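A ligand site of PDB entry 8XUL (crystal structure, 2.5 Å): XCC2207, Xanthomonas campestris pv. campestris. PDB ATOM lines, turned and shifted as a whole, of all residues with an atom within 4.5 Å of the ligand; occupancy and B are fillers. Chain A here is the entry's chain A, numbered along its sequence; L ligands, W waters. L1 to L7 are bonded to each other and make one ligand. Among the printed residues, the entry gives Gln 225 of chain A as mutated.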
ATOM      1  N   ASP A  71      11.057   7.539  27.165  1.00  0.00           N
ATOM      2  CA  ASP A  71       9.744   6.939  27.032  1.00  0.00           C
ATOM      3  C   ASP A  71       9.938   5.541  26.471  1.00  0.00           C
ATOM      4  O   ASP A  71       9.304   4.592  26.910  1.00  0.00           O
ATOM      5  CB  ASP A  71       8.877   7.754  26.074  1.00  0.00           C
ATOM      6  CG  ASP A  71       7.552   7.119  25.702  1.00  0.00           C
ATOM      7  OD1 ASP A  71       6.701   7.015  26.583  1.00  0.00           O
ATOM      8  OD2 ASP A  71       7.380   6.781  24.510  1.00  0.00           O
ATOM      9  N   ARG A  72      10.845   5.454  25.490  1.00  0.00           N
ATOM     10  CA  ARG A  72      11.146   4.206  24.835  1.00  0.00           C
ATOM     11  C   ARG A  72      12.602   4.234  24.378  1.00  0.00           C
ATOM     12  O   ARG A  72      13.175   5.300  24.174  1.00  0.00           O
ATOM     13  CB  ARG A  72      10.139   3.959  23.710  1.00  0.00           C
ATOM     14  CG  ARG A  72       9.870   5.164  22.831  1.00  0.00           C
ATOM     15  CD  ARG A  72       9.222   4.774  21.507  1.00  0.00           C
ATOM     16  NE  ARG A  72       7.819   4.388  21.681  1.00  0.00           N
ATOM     17  CZ  ARG A  72       7.294   3.194  21.476  1.00  0.00           C
ATOM     18  NH1 ARG A  72       7.948   2.257  20.793  1.00  0.00           N
ATOM     19  NH2 ARG A  72       6.069   2.956  21.924  1.00  0.00           N
ATOM     20  N   PHE A  78      12.279  10.995  23.008  1.00  0.00           N
ATOM     21  CA  PHE A  78      12.067  12.034  24.022  1.00  0.00           C
ATOM     22  C   PHE A  78      11.894  11.342  25.372  1.00  0.00           C
ATOM     23  O   PHE A  78      11.688  10.122  25.453  1.00  0.00           O
ATOM     24  CB  PHE A  78      10.880  12.929  23.649  1.00  0.00           C
ATOM     25  CG  PHE A  78       9.643  12.208  23.156  1.00  0.00           C
ATOM     26  CD1 PHE A  78       8.868  11.434  24.011  1.00  0.00           C
ATOM     27  CD2 PHE A  78       9.267  12.267  21.816  1.00  0.00           C
ATOM     28  CE1 PHE A  78       7.760  10.740  23.537  1.00  0.00           C
ATOM     29  CE2 PHE A  78       8.147  11.575  21.354  1.00  0.00           C
ATOM     30  CZ  PHE A  78       7.387  10.821  22.223  1.00  0.00           C
ATOM     31  N   ALA A  82       6.958   9.963  33.602  1.00  0.00           N
ATOM     32  CA  ALA A  82       6.576   8.659  34.120  1.00  0.00           C
ATOM     33  C   ALA A  82       7.756   7.676  34.048  1.00  0.00           C
ATOM     34  O   ALA A  82       7.972   6.931  34.985  1.00  0.00           O
ATOM     35  CB  ALA A  82       5.375   8.133  33.361  1.00  0.00           C
ATOM     36  N   HIS A 137       4.328  15.763  29.931  1.00  0.00           N
ATOM     37  CA  HIS A 137       4.447  14.316  29.891  1.00  0.00           C
ATOM     38  C   HIS A 137       5.783  13.960  29.248  1.00  0.00           C
ATOM     39  O   HIS A 137       6.497  13.067  29.723  1.00  0.00           O
ATOM     40  CB  HIS A 137       3.236  13.776  29.106  1.00  0.00           C
ATOM     41  CG  HIS A 137       3.098  12.297  29.051  1.00  0.00           C
ATOM     42  ND1 HIS A 137       1.919  11.751  28.597  1.00  0.00           N
ATOM     43  CD2 HIS A 137       3.888  11.253  29.350  1.00  0.00           C
ATOM     44  CE1 HIS A 137       2.002  10.427  28.643  1.00  0.00           C
ATOM     45  NE2 HIS A 137       3.184  10.105  29.080  1.00  0.00           N
ATOM     46  N   PHE A 138       6.115  14.691  28.182  1.00  0.00           N
ATOM     47  CA  PHE A 138       7.257  14.375  27.341  1.00  0.00           C
ATOM     48  C   PHE A 138       8.151  15.601  27.236  1.00  0.00           C
ATOM     49  O   PHE A 138       7.691  16.690  26.899  1.00  0.00           O
ATOM     50  CB  PHE A 138       6.781  13.912  25.955  1.00  0.00           C
ATOM     51  CG  PHE A 138       6.032  12.600  26.015  1.00  0.00           C
ATOM     52  CD1 PHE A 138       6.626  11.482  26.574  1.00  0.00           C
ATOM     53  CD2 PHE A 138       4.746  12.497  25.516  1.00  0.00           C
ATOM     54  CE1 PHE A 138       5.946  10.276  26.630  1.00  0.00           C
ATOM     55  CE2 PHE A 138       4.067  11.293  25.581  1.00  0.00           C
ATOM     56  CZ  PHE A 138       4.661  10.192  26.147  1.00  0.00           C
ATOM     57  N   TRP A 150       2.008  19.176  20.891  1.00  0.00           N
ATOM     58  CA  TRP A 150       1.011  18.113  21.057  1.00  0.00           C
ATOM     59  C   TRP A 150       1.086  17.539  22.474  1.00  0.00           C
ATOM     60  O   TRP A 150       0.249  16.730  22.845  1.00  0.00           O
ATOM     61  CB  TRP A 150       1.164  17.005  20.016  1.00  0.00           C
ATOM     62  CG  TRP A 150       2.496  16.324  19.951  1.00  0.00           C
ATOM     63  CD1 TRP A 150       3.475  16.550  19.033  1.00  0.00           C
ATOM     64  CD2 TRP A 150       2.982  15.231  20.765  1.00  0.00           C
ATOM     65  NE1 TRP A 150       4.559  15.761  19.274  1.00  0.00           N
ATOM     66  CE2 TRP A 150       4.275  14.913  20.304  1.00  0.00           C
ATOM     67  CE3 TRP A 150       2.459  14.500  21.841  1.00  0.00           C
ATOM     68  CZ2 TRP A 150       5.052  13.894  20.869  1.00  0.00           C
ATOM     69  CZ3 TRP A 150       3.237  13.513  22.418  1.00  0.00           C
ATOM     70  CH2 TRP A 150       4.512  13.217  21.932  1.00  0.00           C
ATOM     71  N   GLU A 152       0.837  17.360  26.423  1.00  0.00           N
ATOM     72  CA  GLU A 152       0.010  17.865  27.502  1.00  0.00           C
ATOM     73  C   GLU A 152       0.814  17.944  28.809  1.00  0.00           C
ATOM     74  O   GLU A 152       1.755  17.185  28.994  1.00  0.00           O
ATOM     75  CB  GLU A 152      -1.196  16.947  27.672  1.00  0.00           C
ATOM     76  CG  GLU A 152      -0.957  15.707  28.532  1.00  0.00           C
ATOM     77  CD  GLU A 152      -0.236  14.501  27.955  1.00  0.00           C
ATOM     78  OE1 GLU A 152       0.469  14.646  26.923  1.00  0.00           O
ATOM     79  OE2 GLU A 152      -0.407  13.382  28.546  1.00  0.00           O
ATOM     80  N   SER A 154       0.595  16.751  32.268  1.00  0.00           N
ATOM     81  CA  SER A 154      -0.129  15.524  32.615  1.00  0.00           C
ATOM     82  C   SER A 154      -0.216  15.338  34.122  1.00  0.00           C
ATOM     83  O   SER A 154       0.770  15.399  34.852  1.00  0.00           O
ATOM     84  CB  SER A 154       0.503  14.303  32.000  1.00  0.00           C
ATOM     85  OG  SER A 154      -0.280  13.137  32.285  1.00  0.00           O
ATOM     86  N   VAL A 156      -1.690  12.328  35.603  1.00  0.00           N
ATOM     87  CA  VAL A 156      -1.308  10.952  35.891  1.00  0.00           C
ATOM     88  C   VAL A 156       0.207  10.804  35.724  1.00  0.00           C
ATOM     89  O   VAL A 156       0.810  10.018  36.432  1.00  0.00           O
ATOM     90  CB  VAL A 156      -2.061   9.932  35.029  1.00  0.00           C
ATOM     91  CG1 VAL A 156      -1.440   9.783  33.648  1.00  0.00           C
ATOM     92  CG2 VAL A 156      -2.127   8.580  35.692  1.00  0.00           C
ATOM     93  N   ASP A 157       0.809  11.522  34.778  1.00  0.00           N
ATOM     94  CA  ASP A 157       2.222  11.306  34.516  1.00  0.00           C
ATOM     95  C   ASP A 157       3.049  12.036  35.593  1.00  0.00           C
ATOM     96  O   ASP A 157       3.991  11.466  36.134  1.00  0.00           O
ATOM     97  CB  ASP A 157       2.523  11.553  33.031  1.00  0.00           C
ATOM     98  CG  ASP A 157       1.809  10.577  32.081  1.00  0.00           C
ATOM     99  OD1 ASP A 157       2.095   9.349  32.172  1.00  0.00           O
ATOM    100  OD2 ASP A 157       0.971  11.041  31.255  1.00  0.00           O
ATOM    101  N   LEU A 160       2.919   9.708  38.619  1.00  0.00           N
ATOM    102  CA  LEU A 160       3.889   8.615  38.558  1.00  0.00           C
ATOM    103  C   LEU A 160       5.304   9.083  38.945  1.00  0.00           C
ATOM    104  O   LEU A 160       6.009   8.400  39.687  1.00  0.00           O
ATOM    105  CB  LEU A 160       3.890   8.016  37.147  1.00  0.00           C
ATOM    106  CG  LEU A 160       2.666   7.168  36.811  1.00  0.00           C
ATOM    107  CD1 LEU A 160       2.375   7.134  35.321  1.00  0.00           C
ATOM    108  CD2 LEU A 160       2.822   5.743  37.344  1.00  0.00           C
ATOM    109  N   MET A 207      -7.306  15.478  33.346  1.00  0.00           N
ATOM    110  CA  MET A 207      -6.222  14.652  32.836  1.00  0.00           C
ATOM    111  C   MET A 207      -4.982  15.488  32.569  1.00  0.00           C
ATOM    112  O   MET A 207      -3.885  14.942  32.535  1.00  0.00           O
ATOM    113  CB  MET A 207      -6.633  13.945  31.540  1.00  0.00           C
ATOM    114  CG  MET A 207      -7.488  12.740  31.802  1.00  0.00           C
ATOM    115  SD  MET A 207      -7.525  11.554  30.449  1.00  0.00           S
ATOM    116  CE  MET A 207      -8.442  10.262  31.282  1.00  0.00           C
ATOM    117  N   HIS A 218     -11.391  15.513  29.699  1.00  0.00           N
ATOM    118  CA  HIS A 218     -11.521  14.202  30.306  1.00  0.00           C
ATOM    119  C   HIS A 218     -11.001  14.273  31.750  1.00  0.00           C
ATOM    120  O   HIS A 218     -10.064  15.023  32.050  1.00  0.00           O
ATOM    121  CB  HIS A 218     -10.844  13.143  29.434  1.00  0.00           C
ATOM    122  CG  HIS A 218     -11.212  13.238  27.980  1.00  0.00           C
ATOM    123  ND1 HIS A 218     -12.501  13.060  27.502  1.00  0.00           N
ATOM    124  CD2 HIS A 218     -10.459  13.518  26.896  1.00  0.00           C
ATOM    125  CE1 HIS A 218     -12.499  13.210  26.181  1.00  0.00           C
ATOM    126  NE2 HIS A 218     -11.276  13.500  25.792  1.00  0.00           N
ATOM    127  N   TRP A 220     -10.123  11.831  35.478  1.00  0.00           N
ATOM    128  CA  TRP A 220      -9.699  10.527  35.950  1.00  0.00           C
ATOM    129  C   TRP A 220     -10.839   9.913  36.760  1.00  0.00           C
ATOM    130  O   TRP A 220     -11.130  10.368  37.846  1.00  0.00           O
ATOM    131  CB  TRP A 220      -8.387  10.657  36.741  1.00  0.00           C
ATOM    132  CG  TRP A 220      -7.198  10.834  35.845  1.00  0.00           C
ATOM    133  CD1 TRP A 220      -6.469  11.969  35.647  1.00  0.00           C
ATOM    134  CD2 TRP A 220      -6.627   9.839  34.989  1.00  0.00           C
ATOM    135  NE1 TRP A 220      -5.473  11.734  34.728  1.00  0.00           N
ATOM    136  CE2 TRP A 220      -5.542  10.428  34.316  1.00  0.00           C
ATOM    137  CE3 TRP A 220      -6.927   8.496  34.727  1.00  0.00           C
ATOM    138  CZ2 TRP A 220      -4.758   9.733  33.387  1.00  0.00           C
ATOM    139  CZ3 TRP A 220      -6.155   7.805  33.819  1.00  0.00           C
ATOM    140  CH2 TRP A 220      -5.082   8.415  33.173  1.00  0.00           C
ATOM    141  N   ASN A 224      -9.307   2.332  37.032  1.00  0.00           N
ATOM    142  CA  ASN A 224      -8.107   2.274  36.188  1.00  0.00           C
ATOM    143  C   ASN A 224      -6.876   2.464  37.086  1.00  0.00           C
ATOM    144  O   ASN A 224      -6.960   2.223  38.295  1.00  0.00           O
ATOM    145  CB  ASN A 224      -8.176   3.266  35.022  1.00  0.00           C
ATOM    146  CG  ASN A 224      -8.395   4.702  35.430  1.00  0.00           C
ATOM    147  OD1 ASN A 224      -7.688   5.223  36.295  1.00  0.00           O
ATOM    148  ND2 ASN A 224      -9.361   5.358  34.827  1.00  0.00           N
ATOM    149  N   GLN A 225      -5.711   2.783  36.509  1.00  0.00           N
ATOM    150  CA  GLN A 225      -4.428   2.814  37.266  1.00  0.00           C
ATOM    151  C   GLN A 225      -4.189   4.093  38.042  1.00  0.00           C
ATOM    152  O   GLN A 225      -3.116   4.187  38.660  1.00  0.00           O
ATOM    153  CB  GLN A 225      -3.349   2.797  36.185  1.00  0.00           C
ATOM    154  CG  GLN A 225      -3.075   4.157  35.539  1.00  0.00           C
ATOM    155  CD  GLN A 225      -3.925   4.458  34.322  1.00  0.00           C
ATOM    156  OE1 GLN A 225      -5.018   3.928  34.136  1.00  0.00           O
ATOM    157  NE2 GLN A 225      -3.415   5.328  33.469  1.00  0.00           N
ATOM    158  N   PHE A 268     -11.415  -3.824  34.452  1.00  0.00           N
ATOM    159  CA  PHE A 268     -10.674  -2.999  33.493  1.00  0.00           C
ATOM    160  C   PHE A 268      -9.768  -3.942  32.711  1.00  0.00           C
ATOM    161  O   PHE A 268      -9.025  -4.746  33.264  1.00  0.00           O
ATOM    162  CB  PHE A 268      -9.981  -1.877  34.282  1.00  0.00           C
ATOM    163  CG  PHE A 268      -9.136  -0.908  33.512  1.00  0.00           C
ATOM    164  CD1 PHE A 268      -9.709   0.023  32.658  1.00  0.00           C
ATOM    165  CD2 PHE A 268      -7.751  -0.898  33.671  1.00  0.00           C
ATOM    166  CE1 PHE A 268      -8.913   0.899  31.939  1.00  0.00           C
ATOM    167  CE2 PHE A 268      -6.962  -0.014  32.952  1.00  0.00           C
ATOM    168  CZ  PHE A 268      -7.543   0.877  32.087  1.00  0.00           C
ATOM    169  N   PHE A 272      -2.217  -3.332  33.298  1.00  0.00           N
ATOM    170  CA  PHE A 272      -1.441  -2.311  33.990  1.00  0.00           C
ATOM    171  C   PHE A 272      -2.324  -1.512  34.943  1.00  0.00           C
ATOM    172  O   PHE A 272      -1.875  -1.111  36.015  1.00  0.00           O
ATOM    173  CB  PHE A 272      -0.727  -1.370  33.003  1.00  0.00           C
ATOM    174  CG  PHE A 272      -1.509  -0.184  32.487  1.00  0.00           C
ATOM    175  CD1 PHE A 272      -2.403  -0.311  31.432  1.00  0.00           C
ATOM    176  CD2 PHE A 272      -1.323   1.077  33.044  1.00  0.00           C
ATOM    177  CE1 PHE A 272      -3.100   0.795  30.960  1.00  0.00           C
ATOM    178  CE2 PHE A 272      -2.008   2.179  32.551  1.00  0.00           C
ATOM    179  CZ  PHE A 272      -2.906   2.036  31.520  1.00  0.00           C
ATOM    180  N   TYR A 276      -0.035  -0.393  38.350  1.00  0.00           N
ATOM    181  CA  TYR A 276       0.768   0.811  38.563  1.00  0.00           C
ATOM    182  C   TYR A 276       0.668   1.292  40.017  1.00  0.00           C
ATOM    183  O   TYR A 276       1.684   1.379  40.705  1.00  0.00           O
ATOM    184  CB  TYR A 276       0.425   1.932  37.580  1.00  0.00           C
ATOM    185  CG  TYR A 276       0.997   1.775  36.206  1.00  0.00           C
ATOM    186  CD1 TYR A 276       1.571   0.593  35.775  1.00  0.00           C
ATOM    187  CD2 TYR A 276       0.964   2.817  35.304  1.00  0.00           C
ATOM    188  CE1 TYR A 276       2.098   0.447  34.507  1.00  0.00           C
ATOM    189  CE2 TYR A 276       1.466   2.686  34.015  1.00  0.00           C
ATOM    190  CZ  TYR A 276       2.029   1.495  33.608  1.00  0.00           C
ATOM    191  OH  TYR A 276       2.573   1.340  32.361  1.00  0.00           O
ATOM    192  N   TYR A 353       0.932   0.975  18.778  1.00  0.00           N
ATOM    193  CA  TYR A 353       0.796   1.261  20.194  1.00  0.00           C
ATOM    194  C   TYR A 353      -0.687   1.492  20.471  1.00  0.00           C
ATOM    195  O   TYR A 353      -1.337   2.258  19.783  1.00  0.00           O
ATOM    196  CB  TYR A 353       1.671   2.411  20.716  1.00  0.00           C
ATOM    197  CG  TYR A 353       1.569   2.567  22.216  1.00  0.00           C
ATOM    198  CD1 TYR A 353       0.477   3.185  22.804  1.00  0.00           C
ATOM    199  CD2 TYR A 353       2.490   1.958  23.061  1.00  0.00           C
ATOM    200  CE1 TYR A 353       0.336   3.236  24.190  1.00  0.00           C
ATOM    201  CE2 TYR A 353       2.348   2.007  24.438  1.00  0.00           C
ATOM    202  CZ  TYR A 353       1.276   2.646  25.018  1.00  0.00           C
ATOM    203  OH  TYR A 353       1.143   2.706  26.411  1.00  0.00           O
ATOM    204  N   ARG A 361     -14.333  -3.944  29.960  1.00  0.00           N
ATOM    205  CA  ARG A 361     -14.155  -2.644  29.330  1.00  0.00           C
ATOM    206  C   ARG A 361     -12.700  -2.481  28.888  1.00  0.00           C
ATOM    207  O   ARG A 361     -11.790  -2.925  29.606  1.00  0.00           O
ATOM    208  CB  ARG A 361     -14.588  -1.540  30.298  1.00  0.00           C
ATOM    209  CG  ARG A 361     -14.484  -0.132  29.730  1.00  0.00           C
ATOM    210  CD  ARG A 361     -15.089   0.896  30.665  1.00  0.00           C
ATOM    211  NE  ARG A 361     -14.286   1.080  31.871  1.00  0.00           N
ATOM    212  CZ  ARG A 361     -13.215   1.874  31.978  1.00  0.00           C
ATOM    213  NH1 ARG A 361     -12.863   2.667  30.976  1.00  0.00           N
ATOM    214  NH2 ARG A 361     -12.524   1.892  33.106  1.00  0.00           N
ATOM    215  N   GLU A 362     -12.512  -1.831  27.734  1.00  0.00           N
ATOM    216  CA  GLU A 362     -11.213  -1.519  27.134  1.00  0.00           C
ATOM    217  C   GLU A 362     -10.396  -2.801  26.943  1.00  0.00           C
ATOM    218  O   GLU A 362      -9.376  -3.029  27.601  1.00  0.00           O
ATOM    219  CB  GLU A 362     -10.464  -0.477  27.969  1.00  0.00           C
ATOM    220  CG  GLU A 362      -9.591   0.435  27.119  1.00  0.00           C
ATOM    221  CD  GLU A 362      -8.892   1.532  27.893  1.00  0.00           C
ATOM    222  OE1 GLU A 362      -7.661   1.522  27.949  1.00  0.00           O
ATOM    223  OE2 GLU A 362      -9.591   2.411  28.419  1.00  0.00           O
ATOM    224  N   ILE A 437       9.640  -0.190  26.590  1.00  0.00           N
ATOM    225  CA  ILE A 437       8.878   0.970  27.058  1.00  0.00           C
ATOM    226  C   ILE A 437       9.071   1.065  28.573  1.00  0.00           C
ATOM    227  O   ILE A 437       8.809   0.100  29.268  1.00  0.00           O
ATOM    228  CB  ILE A 437       7.392   0.829  26.674  1.00  0.00           C
ATOM    229  CG1 ILE A 437       7.235   0.682  25.148  1.00  0.00           C
ATOM    230  CG2 ILE A 437       6.585   1.998  27.239  1.00  0.00           C
ATOM    231  CD1 ILE A 437       5.820   0.839  24.635  1.00  0.00           C
ATOM    232  N   ILE A 439       7.607   2.582  31.114  1.00  0.00           N
ATOM    233  CA  ILE A 439       6.442   2.366  31.966  1.00  0.00           C
ATOM    234  C   ILE A 439       5.964   0.910  31.869  1.00  0.00           C
ATOM    235  O   ILE A 439       5.131   0.498  32.664  1.00  0.00           O
ATOM    236  CB  ILE A 439       5.315   3.362  31.633  1.00  0.00           C
ATOM    237  CG1 ILE A 439       4.720   3.141  30.247  1.00  0.00           C
ATOM    238  CG2 ILE A 439       5.796   4.804  31.817  1.00  0.00           C
ATOM    239  CD1 ILE A 439       3.363   3.774  30.079  1.00  0.00           C
HETATM  240  C1  LIG L   1      -7.939   8.597  27.343  1.00  0.00           C
HETATM  241  C2  LIG L   1      -7.275   9.806  26.716  1.00  0.00           C
HETATM  242  C3  LIG L   1      -7.932  10.171  25.398  1.00  0.00           C
HETATM  243  C4  LIG L   1      -9.447  10.274  25.556  1.00  0.00           C
HETATM  244  C5  LIG L   1     -10.143  10.445  24.232  1.00  0.00           C
HETATM  245  C6  LIG L   1      -9.428   8.793  27.432  1.00  0.00           C
HETATM  246  O1  LIG L   1     -10.055   7.669  27.959  1.00  0.00           O
HETATM  247  O2  LIG L   1      -7.388   8.350  28.631  1.00  0.00           O
HETATM  248  O3  LIG L   1      -5.899   9.526  26.496  1.00  0.00           O
HETATM  249  O4  LIG L   1      -7.439  11.429  24.964  1.00  0.00           O
HETATM  250  O5  LIG L   1      -9.945   9.061  26.135  1.00  0.00           O
HETATM  251  O6  LIG L   1     -11.542  10.620  24.421  1.00  0.00           O
HETATM  252  C1  LG2 L   2      -5.698   7.105  29.657  1.00  0.00           C
HETATM  253  C2  LG2 L   2      -5.307   5.747  30.209  1.00  0.00           C
HETATM  254  C3  LG2 L   2      -6.428   5.223  31.077  1.00  0.00           C
HETATM  255  C4  LG2 L   2      -7.701   5.148  30.267  1.00  0.00           C
HETATM  256  C5  LG2 L   2      -8.880   4.701  31.078  1.00  0.00           C
HETATM  257  C6  LG2 L   2      -7.019   7.036  28.934  1.00  0.00           C
HETATM  258  O1  LG2 L   2      -4.691   7.608  28.787  1.00  0.00           O
HETATM  259  O2  LG2 L   2      -4.106   5.869  30.962  1.00  0.00           O
HETATM  260  O3  LG2 L   2      -6.110   3.924  31.559  1.00  0.00           O
HETATM  261  O4  LG2 L   2      -8.028   6.465  29.771  1.00  0.00           O
HETATM  262  O5  LG2 L   2      -9.933   4.223  30.249  1.00  0.00           O
HETATM  263  C1  LG3 L   3      -2.604   8.726  29.259  1.00  0.00           C
HETATM  264  C2  LG3 L   3      -2.078   9.974  29.917  1.00  0.00           C
HETATM  265  C3  LG3 L   3      -2.646  11.206  29.230  1.00  0.00           C
HETATM  266  C4  LG3 L   3      -4.166  11.154  29.191  1.00  0.00           C
HETATM  267  C5  LG3 L   3      -4.766  12.271  28.383  1.00  0.00           C
HETATM  268  C6  LG3 L   3      -4.112   8.770  29.276  1.00  0.00           C
HETATM  269  O1  LG3 L   3      -2.133   7.562  29.917  1.00  0.00           O
HETATM  270  O2  LG3 L   3      -0.663   9.984  29.844  1.00  0.00           O
HETATM  271  O3  LG3 L   3      -2.248  12.365  29.937  1.00  0.00           O
HETATM  272  O4  LG3 L   3      -4.578   9.919  28.590  1.00  0.00           O
HETATM  273  O5  LG3 L   3      -3.939  12.617  27.283  1.00  0.00           O
HETATM  274  C1  LG4 L   4      -0.449   7.083  28.186  1.00  0.00           C
HETATM  275  C2  LG4 L   4       0.964   6.789  28.601  1.00  0.00           C
HETATM  276  C3  LG4 L   4       1.091   7.104  30.074  1.00  0.00           C
HETATM  277  C4  LG4 L   4       0.335   6.042  30.859  1.00  0.00           C
HETATM  278  C5  LG4 L   4      -0.133   6.520  32.208  1.00  0.00           C
HETATM  279  C6  LG4 L   4      -1.429   6.576  29.231  1.00  0.00           C
HETATM  280  O1  LG4 L   4      -0.687   6.468  26.930  1.00  0.00           O
HETATM  281  O2  LG4 L   4       1.878   7.548  27.828  1.00  0.00           O
HETATM  282  O3  LG4 L   4       2.459   7.130  30.460  1.00  0.00           O
HETATM  283  O4  LG4 L   4      -0.837   5.609  30.114  1.00  0.00           O
HETATM  284  O5  LG4 L   4      -0.649   5.433  32.963  1.00  0.00           O
HETATM  285  C1  LG5 L   5      -0.928   7.018  24.673  1.00  0.00           C
HETATM  286  C2  LG5 L   5      -1.893   7.502  23.617  1.00  0.00           C
HETATM  287  C3  LG5 L   5      -3.286   6.939  23.837  1.00  0.00           C
HETATM  288  C4  LG5 L   5      -3.747   7.167  25.263  1.00  0.00           C
HETATM  289  C5  LG5 L   5      -5.059   6.465  25.553  1.00  0.00           C
HETATM  290  C6  LG5 L   5      -1.499   7.193  26.063  1.00  0.00           C
HETATM  291  O1  LG5 L   5       0.319   7.690  24.565  1.00  0.00           O
HETATM  292  O2  LG5 L   5      -1.414   7.133  22.321  1.00  0.00           O
HETATM  293  O3  LG5 L   5      -4.198   7.599  22.967  1.00  0.00           O
HETATM  294  O4  LG5 L   5      -2.793   6.602  26.155  1.00  0.00           O
HETATM  295  O5  LG5 L   5      -4.873   5.057  25.673  1.00  0.00           O
HETATM  296  C1  LG6 L   6       2.277   7.687  23.197  1.00  0.00           C
HETATM  297  C2  LG6 L   6       3.501   6.884  22.801  1.00  0.00           C
HETATM  298  C3  LG6 L   6       4.209   6.336  24.027  1.00  0.00           C
HETATM  299  C4  LG6 L   6       3.248   5.638  24.955  1.00  0.00           C
HETATM  300  C5  LG6 L   6       3.890   5.208  26.251  1.00  0.00           C
HETATM  301  C6  LG6 L   6       1.400   6.923  24.164  1.00  0.00           C
HETATM  302  O1  LG6 L   6       1.531   8.055  22.044  1.00  0.00           O
HETATM  303  O2  LG6 L   6       4.380   7.714  22.054  1.00  0.00           O
HETATM  304  O3  LG6 L   6       5.201   5.394  23.621  1.00  0.00           O
HETATM  305  O4  LG6 L   6       2.186   6.537  25.297  1.00  0.00           O
HETATM  306  O5  LG6 L   6       4.281   6.338  27.018  1.00  0.00           O
HETATM  307  C1  LG7 L   7       1.688   9.800  20.442  1.00  0.00           C
HETATM  308  C2  LG7 L   7       1.348  11.256  20.170  1.00  0.00           C
HETATM  309  C3  LG7 L   7      -0.078  11.540  20.582  1.00  0.00           C
HETATM  310  C4  LG7 L   7      -0.281  11.157  22.030  1.00  0.00           C
HETATM  311  C5  LG7 L   7      -1.706  11.344  22.489  1.00  0.00           C
HETATM  312  C6  LG7 L   7       1.368   9.421  21.870  1.00  0.00           C
HETATM  313  O1  LG7 L   7       3.056   9.546  20.154  1.00  0.00           O
HETATM  314  O2  LG7 L   7       1.546  11.553  18.788  1.00  0.00           O
HETATM  315  O3  LG7 L   7      -0.367  12.920  20.429  1.00  0.00           O
HETATM  316  O4  LG7 L   7       0.023   9.764  22.185  1.00  0.00           O
HETATM  317  O5  LG7 L   7      -2.622  11.015  21.448  1.00  0.00           O
HETATM  318  O   HOH W   1      -3.205  12.487  32.726  1.00  0.00           O
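A ring nitrogen (ND1) of His 137 sits close to the side-chain carboxylate of Asp 157 (2.9 Å).
The side-chain hydroxyl of Ser 154 lies within hydrogen-bond range of the side-chain carboxylate of Asp 157 (2.6 Å).
OE2 of Glu 152 is in hydrogen-bond range of ND1 of His 137.
The side-chain carboxylate (OD2) of Asp 71 lies within salt-bridge range of the guanidinium group (NE) of Arg 72, at 3.7 Å.
The backbone NH of Asp 71 sits at hydrogen-bond distance from the backbone carbonyl oxygen of Phe 78, at 3.2 Å.
The backbone NH (N) of Met 207 lies within hydrogen-bond range of the backbone carbonyl oxygen (O) of His 218 (3.1 Å).
O of Ile 439 sits at hydrogen-bond distance from OH of Tyr 276 (2.7 Å).
O2 of LG3 L3 is in hydrogen-bond range of OD2 of Asp 157.
The side-chain carboxylate (OE2) of Glu 152 sits at hydrogen-bond distance from an oxygen (O3) of LG3 L3, 2.5 Å away.
OD1 of Asp 71 lies within hydrogen-bond range of O5 of LG6 L6 (2.6 Å).
O5 of LG2 L2 sits at hydrogen-bond distance from OE2 of Glu 362 (2.6 Å).
An oxygen (O2) of LG2 L2 sits at hydrogen-bond distance from the side-chain amide nitrogen (NE2) of Gln 225, 2.7 Å away.
An oxygen (O2) of LG4 L4 lies close to a ring nitrogen (NE2) of His 137, at 3.1 Å.
NH2 of Arg 72 is in hydrogen-bond range of O3 of LG6 L6, 3.1 Å away.
The side-chain hydroxyl (OG) of Ser 154 sits at hydrogen-bond distance from an oxygen (O3) of LG3 L3 (3.2 Å).
NE2 of His 218 is in hydrogen-bond range of O6 of LIG L1 (3.2 Å).
The guanidinium group (NH1) of Arg 361 sits at hydrogen-bond distance from an oxygen (O5) of LG2 L2, at 3.4 Å.
Water W1 lies within hydrogen-bond range of the backbone carbonyl oxygen of Met 207, an oxygen (O3) of LG3 L3, the side-chain hydroxyl of Ser 154, the indole nitrogen of Trp 220 and the backbone NH of Val 156.
The side-chain sulfur of Met 207 sits close to an oxygen (O2) of LIG L1.
CZ of Phe 138 touches O5 of LG6 L6 (3.97 Å).
CE3 of Trp 150 touches O3 of LG7 L7, 3.5 Å away.
Val 156 touches the ligand.
Trp 220 touches the ligand.
Asn 224 touches the ligand.
CZ of Phe 268 touches O3 of LG2 L2, 3.4 Å away.
CE2 of Phe 272 touches O5 of LG4 L4, 3.6 Å away.
CE2 of Tyr 276 touches O5 of LG4 L4 (3.6 Å).
CZ of Tyr 353 touches C4 of LG6 L6, at 3.6 Å.
Ile 439 touches the ligand.
Hydrophobic or aromatic side chains within 4 Å of the ligand: His 137, Phe 138, Trp 150, Val 156, Met 207, His 218, Trp 220, Phe 268, Phe 272, Tyr 276, Tyr 353 and Ile 439.
21 residues have an atom within 4 Å of the ligand: Asp 71, Arg 72, His 137, Phe 138, Trp 150, Glu 152, Ser 154, Val 156, Asp 157, Met 207, His 218, Trp 220, Asn 224, Gln 225, Phe 268, Phe 272, Tyr 276, Tyr 353, Arg 361, Glu 362 and Ile 439.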
